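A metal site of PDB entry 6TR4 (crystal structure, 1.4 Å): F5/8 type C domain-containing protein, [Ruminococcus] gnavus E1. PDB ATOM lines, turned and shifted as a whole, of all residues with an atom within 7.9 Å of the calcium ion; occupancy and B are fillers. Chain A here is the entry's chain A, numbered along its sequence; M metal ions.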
ATOM      1  N   LYS A 394       3.270 -12.005  23.120  1.00  0.00           N
ATOM      2  CA  LYS A 394       3.334 -12.869  24.324  1.00  0.00           C
ATOM      3  C   LYS A 394       3.635 -12.049  25.575  1.00  0.00           C
ATOM      4  O   LYS A 394       4.267 -10.982  25.505  1.00  0.00           O
ATOM      5  CB  LYS A 394       4.374 -13.956  24.127  1.00  0.00           C
ATOM      6  CG  LYS A 394       5.827 -13.487  24.170  1.00  0.00           C
ATOM      7  CD  LYS A 394       6.798 -14.598  23.814  1.00  0.00           C
ATOM      8  CE  LYS A 394       8.227 -14.144  23.921  1.00  0.00           C
ATOM      9  NZ  LYS A 394       9.183 -15.253  23.671  1.00  0.00           N
ATOM     10  N   PRO A 395       3.184 -12.497  26.771  1.00  0.00           N
ATOM     11  CA  PRO A 395       3.440 -11.767  27.998  1.00  0.00           C
ATOM     12  C   PRO A 395       4.925 -11.597  28.334  1.00  0.00           C
ATOM     13  O   PRO A 395       5.292 -10.605  28.936  1.00  0.00           O
ATOM     14  CB  PRO A 395       2.706 -12.566  29.082  1.00  0.00           C
ATOM     15  CG  PRO A 395       2.504 -13.932  28.472  1.00  0.00           C
ATOM     16  CD  PRO A 395       2.344 -13.683  26.986  1.00  0.00           C
ATOM     17  N   GLY A 396       5.768 -12.545  27.922  1.00  0.00           N
ATOM     18  CA  GLY A 396       7.219 -12.441  28.154  1.00  0.00           C
ATOM     19  C   GLY A 396       7.813 -11.241  27.456  1.00  0.00           C
ATOM     20  O   GLY A 396       8.930 -10.832  27.797  1.00  0.00           O
ATOM     21  N   ASN A 397       7.109 -10.651  26.485  1.00  0.00           N
ATOM     22  CA  ASN A 397       7.537  -9.383  25.858  1.00  0.00           C
ATOM     23  C   ASN A 397       7.579  -8.262  26.897  1.00  0.00           C
ATOM     24  O   ASN A 397       8.224  -7.239  26.606  1.00  0.00           O
ATOM     25  CB  ASN A 397       6.623  -8.967  24.719  1.00  0.00           C
ATOM     26  CG  ASN A 397       6.844  -9.777  23.477  1.00  0.00           C
ATOM     27  OD1 ASN A 397       7.780 -10.557  23.385  1.00  0.00           O
ATOM     28  ND2 ASN A 397       5.995  -9.565  22.494  1.00  0.00           N
ATOM     29  N   MET A 398       6.967  -8.415  28.068  1.00  0.00           N
ATOM     30  CA  MET A 398       6.954  -7.334  29.082  1.00  0.00           C
ATOM     31  C   MET A 398       8.159  -7.488  30.023  1.00  0.00           C
ATOM     32  O   MET A 398       8.330  -6.631  30.896  1.00  0.00           O
ATOM     33  CB  MET A 398       5.644  -7.353  29.865  1.00  0.00           C
ATOM     34  CG  MET A 398       4.461  -6.994  29.005  1.00  0.00           C
ATOM     35  SD  MET A 398       2.925  -6.889  29.926  1.00  0.00           S
ATOM     36  CE  MET A 398       2.498  -8.622  30.035  1.00  0.00           C
ATOM     37  N   ILE A 399       8.997  -8.510  29.869  1.00  0.00           N
ATOM     38  CA  ILE A 399      10.137  -8.715  30.811  1.00  0.00           C
ATOM     39  C   ILE A 399      11.392  -9.071  30.008  1.00  0.00           C
ATOM     40  O   ILE A 399      12.272  -9.723  30.562  1.00  0.00           O
ATOM     41  CB  ILE A 399       9.798  -9.761  31.898  1.00  0.00           C
ATOM     42  CG1 ILE A 399       9.257 -11.051  31.283  1.00  0.00           C
ATOM     43  CG2 ILE A 399       8.832  -9.159  32.931  1.00  0.00           C
ATOM     44  CD1 ILE A 399       9.190 -12.210  32.269  1.00  0.00           C
ATOM     45  N   ASP A 400      11.491  -8.620  28.750  1.00  0.00           N
ATOM     46  CA  ASP A 400      12.654  -8.950  27.903  1.00  0.00           C
ATOM     47  C   ASP A 400      13.604  -7.753  27.783  1.00  0.00           C
ATOM     48  O   ASP A 400      14.591  -7.894  27.070  1.00  0.00           O
ATOM     49  CB  ASP A 400      12.227  -9.487  26.544  1.00  0.00           C
ATOM     50  CG  ASP A 400      11.474  -8.504  25.674  1.00  0.00           C
ATOM     51  OD1 ASP A 400      11.143  -7.393  26.184  1.00  0.00           O
ATOM     52  OD2 ASP A 400      11.182  -8.864  24.506  1.00  0.00           O
ATOM     53  N   ASP A 401      13.351  -6.634  28.469  1.00  0.00           N
ATOM     54  CA  ASP A 401      14.281  -5.467  28.475  1.00  0.00           C
ATOM     55  C   ASP A 401      14.480  -4.986  27.043  1.00  0.00           C
ATOM     56  O   ASP A 401      15.584  -4.542  26.678  1.00  0.00           O
ATOM     57  CB  ASP A 401      15.596  -5.819  29.178  1.00  0.00           C
ATOM     58  CG  ASP A 401      15.434  -5.904  30.696  1.00  0.00           C
ATOM     59  OD1 ASP A 401      14.715  -5.060  31.271  1.00  0.00           O
ATOM     60  OD2 ASP A 401      15.982  -6.817  31.269  1.00  0.00           O
ATOM     61  N   ASN A 402      13.423  -5.041  26.254  1.00  0.00           N
ATOM     62  CA  ASN A 402      13.403  -4.580  24.851  1.00  0.00           C
ATOM     63  C   ASN A 402      12.174  -3.699  24.679  1.00  0.00           C
ATOM     64  O   ASN A 402      11.042  -4.210  24.708  1.00  0.00           O
ATOM     65  CB  ASN A 402      13.401  -5.758  23.876  1.00  0.00           C
ATOM     66  CG  ASN A 402      13.385  -5.355  22.421  1.00  0.00           C
ATOM     67  OD1 ASN A 402      13.186  -4.191  22.096  1.00  0.00           O
ATOM     68  ND2 ASN A 402      13.503  -6.344  21.535  1.00  0.00           N
ATOM     69  N   ASP A 403      12.368  -2.397  24.524  1.00  0.00           N
ATOM     70  CA  ASP A 403      11.243  -1.453  24.423  1.00  0.00           C
ATOM     71  C   ASP A 403      10.439  -1.683  23.147  1.00  0.00           C
ATOM     72  O   ASP A 403       9.297  -1.222  23.096  1.00  0.00           O
ATOM     73  CB  ASP A 403      11.740  -0.010  24.414  1.00  0.00           C
ATOM     74  CG  ASP A 403      12.378   0.437  25.712  1.00  0.00           C
ATOM     75  OD1 ASP A 403      12.134  -0.199  26.772  1.00  0.00           O
ATOM     76  OD2 ASP A 403      13.142   1.419  25.650  1.00  0.00           O
ATOM     77  N   GLU A 404      10.986  -2.384  22.148  1.00  0.00           N
ATOM     78  CA  GLU A 404      10.280  -2.568  20.855  1.00  0.00           C
ATOM     79  C   GLU A 404       9.269  -3.724  20.930  1.00  0.00           C
ATOM     80  O   GLU A 404       8.382  -3.765  20.089  1.00  0.00           O
ATOM     81  CB  GLU A 404      11.289  -2.773  19.729  1.00  0.00           C
ATOM     82  CG  GLU A 404      12.146  -1.541  19.489  1.00  0.00           C
ATOM     83  CD  GLU A 404      11.376  -0.305  19.054  1.00  0.00           C
ATOM     84  OE1 GLU A 404      10.472  -0.457  18.195  1.00  0.00           O
ATOM     85  OE2 GLU A 404      11.651   0.824  19.570  1.00  0.00           O
ATOM     86  N   THR A 405       9.396  -4.610  21.904  1.00  0.00           N
ATOM     87  CA  THR A 405       8.450  -5.752  22.040  1.00  0.00           C
ATOM     88  C   THR A 405       7.422  -5.449  23.120  1.00  0.00           C
ATOM     89  O   THR A 405       7.770  -4.921  24.194  1.00  0.00           O
ATOM     90  CB  THR A 405       9.174  -7.055  22.378  1.00  0.00           C
ATOM     91  OG1 THR A 405       9.792  -6.878  23.665  1.00  0.00           O
ATOM     92  CG2 THR A 405      10.199  -7.455  21.332  1.00  0.00           C
ATOM     93  N   TYR A 406       6.171  -5.784  22.870  1.00  0.00           N
ATOM     94  CA  TYR A 406       5.101  -5.503  23.835  1.00  0.00           C
ATOM     95  C   TYR A 406       4.068  -6.627  23.813  1.00  0.00           C
ATOM     96  O   TYR A 406       3.974  -7.424  22.858  1.00  0.00           O
ATOM     97  CB  TYR A 406       4.465  -4.146  23.529  1.00  0.00           C
ATOM     98  CG  TYR A 406       3.991  -3.971  22.109  1.00  0.00           C
ATOM     99  CD1 TYR A 406       2.711  -4.328  21.737  1.00  0.00           C
ATOM    100  CD2 TYR A 406       4.812  -3.406  21.135  1.00  0.00           C
ATOM    101  CE1 TYR A 406       2.266  -4.160  20.436  1.00  0.00           C
ATOM    102  CE2 TYR A 406       4.384  -3.252  19.835  1.00  0.00           C
ATOM    103  CZ  TYR A 406       3.099  -3.625  19.486  1.00  0.00           C
ATOM    104  OH  TYR A 406       2.656  -3.481  18.202  1.00  0.00           O
ATOM    105  N   TRP A 407       3.329  -6.674  24.921  1.00  0.00           N
ATOM    106  CA  TRP A 407       2.063  -7.424  25.037  1.00  0.00           C
ATOM    107  C   TRP A 407       0.922  -6.522  24.574  1.00  0.00           C
ATOM    108  O   TRP A 407       0.960  -5.303  24.810  1.00  0.00           O
ATOM    109  CB  TRP A 407       1.861  -7.945  26.454  1.00  0.00           C
ATOM    110  CG  TRP A 407       0.449  -8.361  26.741  1.00  0.00           C
ATOM    111  CD1 TRP A 407      -0.192  -9.466  26.292  1.00  0.00           C
ATOM    112  CD2 TRP A 407      -0.506  -7.622  27.520  1.00  0.00           C
ATOM    113  NE1 TRP A 407      -1.492  -9.465  26.732  1.00  0.00           N
ATOM    114  CE2 TRP A 407      -1.717  -8.353  27.481  1.00  0.00           C
ATOM    115  CE3 TRP A 407      -0.480  -6.408  28.202  1.00  0.00           C
ATOM    116  CZ2 TRP A 407      -2.852  -7.917  28.162  1.00  0.00           C
ATOM    117  CZ3 TRP A 407      -1.606  -5.970  28.869  1.00  0.00           C
ATOM    118  CH2 TRP A 407      -2.782  -6.725  28.855  1.00  0.00           C
ATOM    119  N   GLU A 434       5.376   0.270  31.663  1.00  0.00           N
ATOM    120  CA  GLU A 434       5.777   1.124  30.514  1.00  0.00           C
ATOM    121  C   GLU A 434       4.880   0.802  29.347  1.00  0.00           C
ATOM    122  O   GLU A 434       4.900  -0.352  28.883  1.00  0.00           O
ATOM    123  CB  GLU A 434       7.255   0.910  30.202  1.00  0.00           C
ATOM    124  CG  GLU A 434       8.166   1.218  31.362  1.00  0.00           C
ATOM    125  CD  GLU A 434       9.623   0.861  31.107  1.00  0.00           C
ATOM    126  OE1 GLU A 434      10.163   1.214  30.047  1.00  0.00           O
ATOM    127  OE2 GLU A 434      10.222   0.250  32.013  1.00  0.00           O
ATOM    128  N   GLN A 438       5.828   4.411  21.465  1.00  0.00           N
ATOM    129  CA  GLN A 438       6.156   4.551  20.034  1.00  0.00           C
ATOM    130  C   GLN A 438       4.894   4.439  19.176  1.00  0.00           C
ATOM    131  O   GLN A 438       4.868   4.995  18.052  1.00  0.00           O
ATOM    132  CB  GLN A 438       7.243   3.564  19.608  1.00  0.00           C
ATOM    133  CG  GLN A 438       6.881   2.092  19.741  1.00  0.00           C
ATOM    134  CD  GLN A 438       7.245   1.445  21.056  1.00  0.00           C
ATOM    135  OE1 GLN A 438       7.130   2.020  22.122  1.00  0.00           O
ATOM    136  NE2 GLN A 438       7.692   0.189  20.983  1.00  0.00           N
ATOM    137  N   ILE A 497       1.791  -2.843  26.192  1.00  0.00           N
ATOM    138  CA  ILE A 497       2.733  -2.689  27.331  1.00  0.00           C
ATOM    139  C   ILE A 497       4.079  -3.257  26.937  1.00  0.00           C
ATOM    140  O   ILE A 497       4.145  -4.455  26.656  1.00  0.00           O
ATOM    141  CB  ILE A 497       2.191  -3.360  28.608  1.00  0.00           C
ATOM    142  CG1 ILE A 497       0.846  -2.772  29.027  1.00  0.00           C
ATOM    143  CG2 ILE A 497       3.239  -3.279  29.713  1.00  0.00           C
ATOM    144  CD1 ILE A 497       0.881  -1.341  29.444  1.00  0.00           C
ATOM    145  N   SER A 498       5.119  -2.426  26.899  1.00  0.00           N
ATOM    146  CA  SER A 498       6.452  -2.880  26.436  1.00  0.00           C
ATOM    147  C   SER A 498       7.269  -3.481  27.575  1.00  0.00           C
ATOM    148  O   SER A 498       8.095  -4.366  27.288  1.00  0.00           O
ATOM    149  CB  SER A 498       7.195  -1.794  25.690  1.00  0.00           C
ATOM    150  OG  SER A 498       7.152  -0.565  26.361  1.00  0.00           O
ATOM    151  N   GLU A 499       7.100  -3.013  28.818  1.00  0.00           N
ATOM    152  CA  GLU A 499       7.884  -3.558  29.958  1.00  0.00           C
ATOM    153  C   GLU A 499       7.084  -3.398  31.238  1.00  0.00           C
ATOM    154  O   GLU A 499       6.336  -2.403  31.382  1.00  0.00           O
ATOM    155  CB  GLU A 499       9.235  -2.862  30.117  1.00  0.00           C
ATOM    156  CG  GLU A 499      10.228  -3.095  28.983  1.00  0.00           C
ATOM    157  CD  GLU A 499      10.724  -4.507  28.738  1.00  0.00           C
ATOM    158  OE1 GLU A 499      10.998  -5.287  29.725  1.00  0.00           O
ATOM    159  OE2 GLU A 499      10.833  -4.863  27.568  1.00  0.00           O
ATOM    160  N   ILE A 500       7.239  -4.335  32.161  1.00  0.00           N
ATOM    161  CA  ILE A 500       6.773  -4.187  33.566  1.00  0.00           C
ATOM    162  C   ILE A 500       7.877  -4.661  34.493  1.00  0.00           C
ATOM    163  O   ILE A 500       8.760  -5.430  34.073  1.00  0.00           O
ATOM    164  CB  ILE A 500       5.477  -4.963  33.836  1.00  0.00           C
ATOM    165  CG1 ILE A 500       5.716  -6.475  33.749  1.00  0.00           C
ATOM    166  CG2 ILE A 500       4.365  -4.491  32.924  1.00  0.00           C
ATOM    167  CD1 ILE A 500       4.472  -7.297  33.869  1.00  0.00           C
HETATM  168 CA    CA M   1       9.521  -5.599  25.788  1.00  0.00          CA
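Six residues have an atom within 4 Å of the calcium ion: Asn 397, Asp 400, Asn 402, Thr 405, Ser 498 and Glu 499.
The calcium ion is bound by the backbone carbonyl oxygen of Asn 397 (2.2 Å), the backbone carbonyl oxygen of Asn 402 (2.3 Å), the side-chain carboxylate of Glu 499 (2.3 Å), the backbone carbonyl oxygen of Ser 498 (2.4 Å), the side-chain carboxylate of Asp 400 (2.5 Å), the backbone carbonyl oxygen of Thr 405 (2.5 Å) and the side-chain hydroxyl of Thr 405 (2.5 Å).
The calcium ion has seven donor atoms within binding distance.
The side-chain amide nitrogen (ND2) of Asn 397 lies within hydrogen-bond range of the backbone carbonyl oxygen (O) of Tyr 406.
The side-chain amide oxygen (OD1) of Asn 402 sits at hydrogen-bond distance from the backbone NH (N) of Glu 404 (2.8 Å).
The side-chain carboxylate (OE1) of Glu 499 sits at hydrogen-bond distance from the backbone NH (N) of Asp 401, 3.0 Å away.
The backbone carbonyl oxygen (O) of Glu 499 is in hydrogen-bond range of the backbone NH (N) of Glu 434 (2.9 Å).
N of Ser 498 lies within hydrogen-bond range of O of Glu 434 (2.9 Å).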
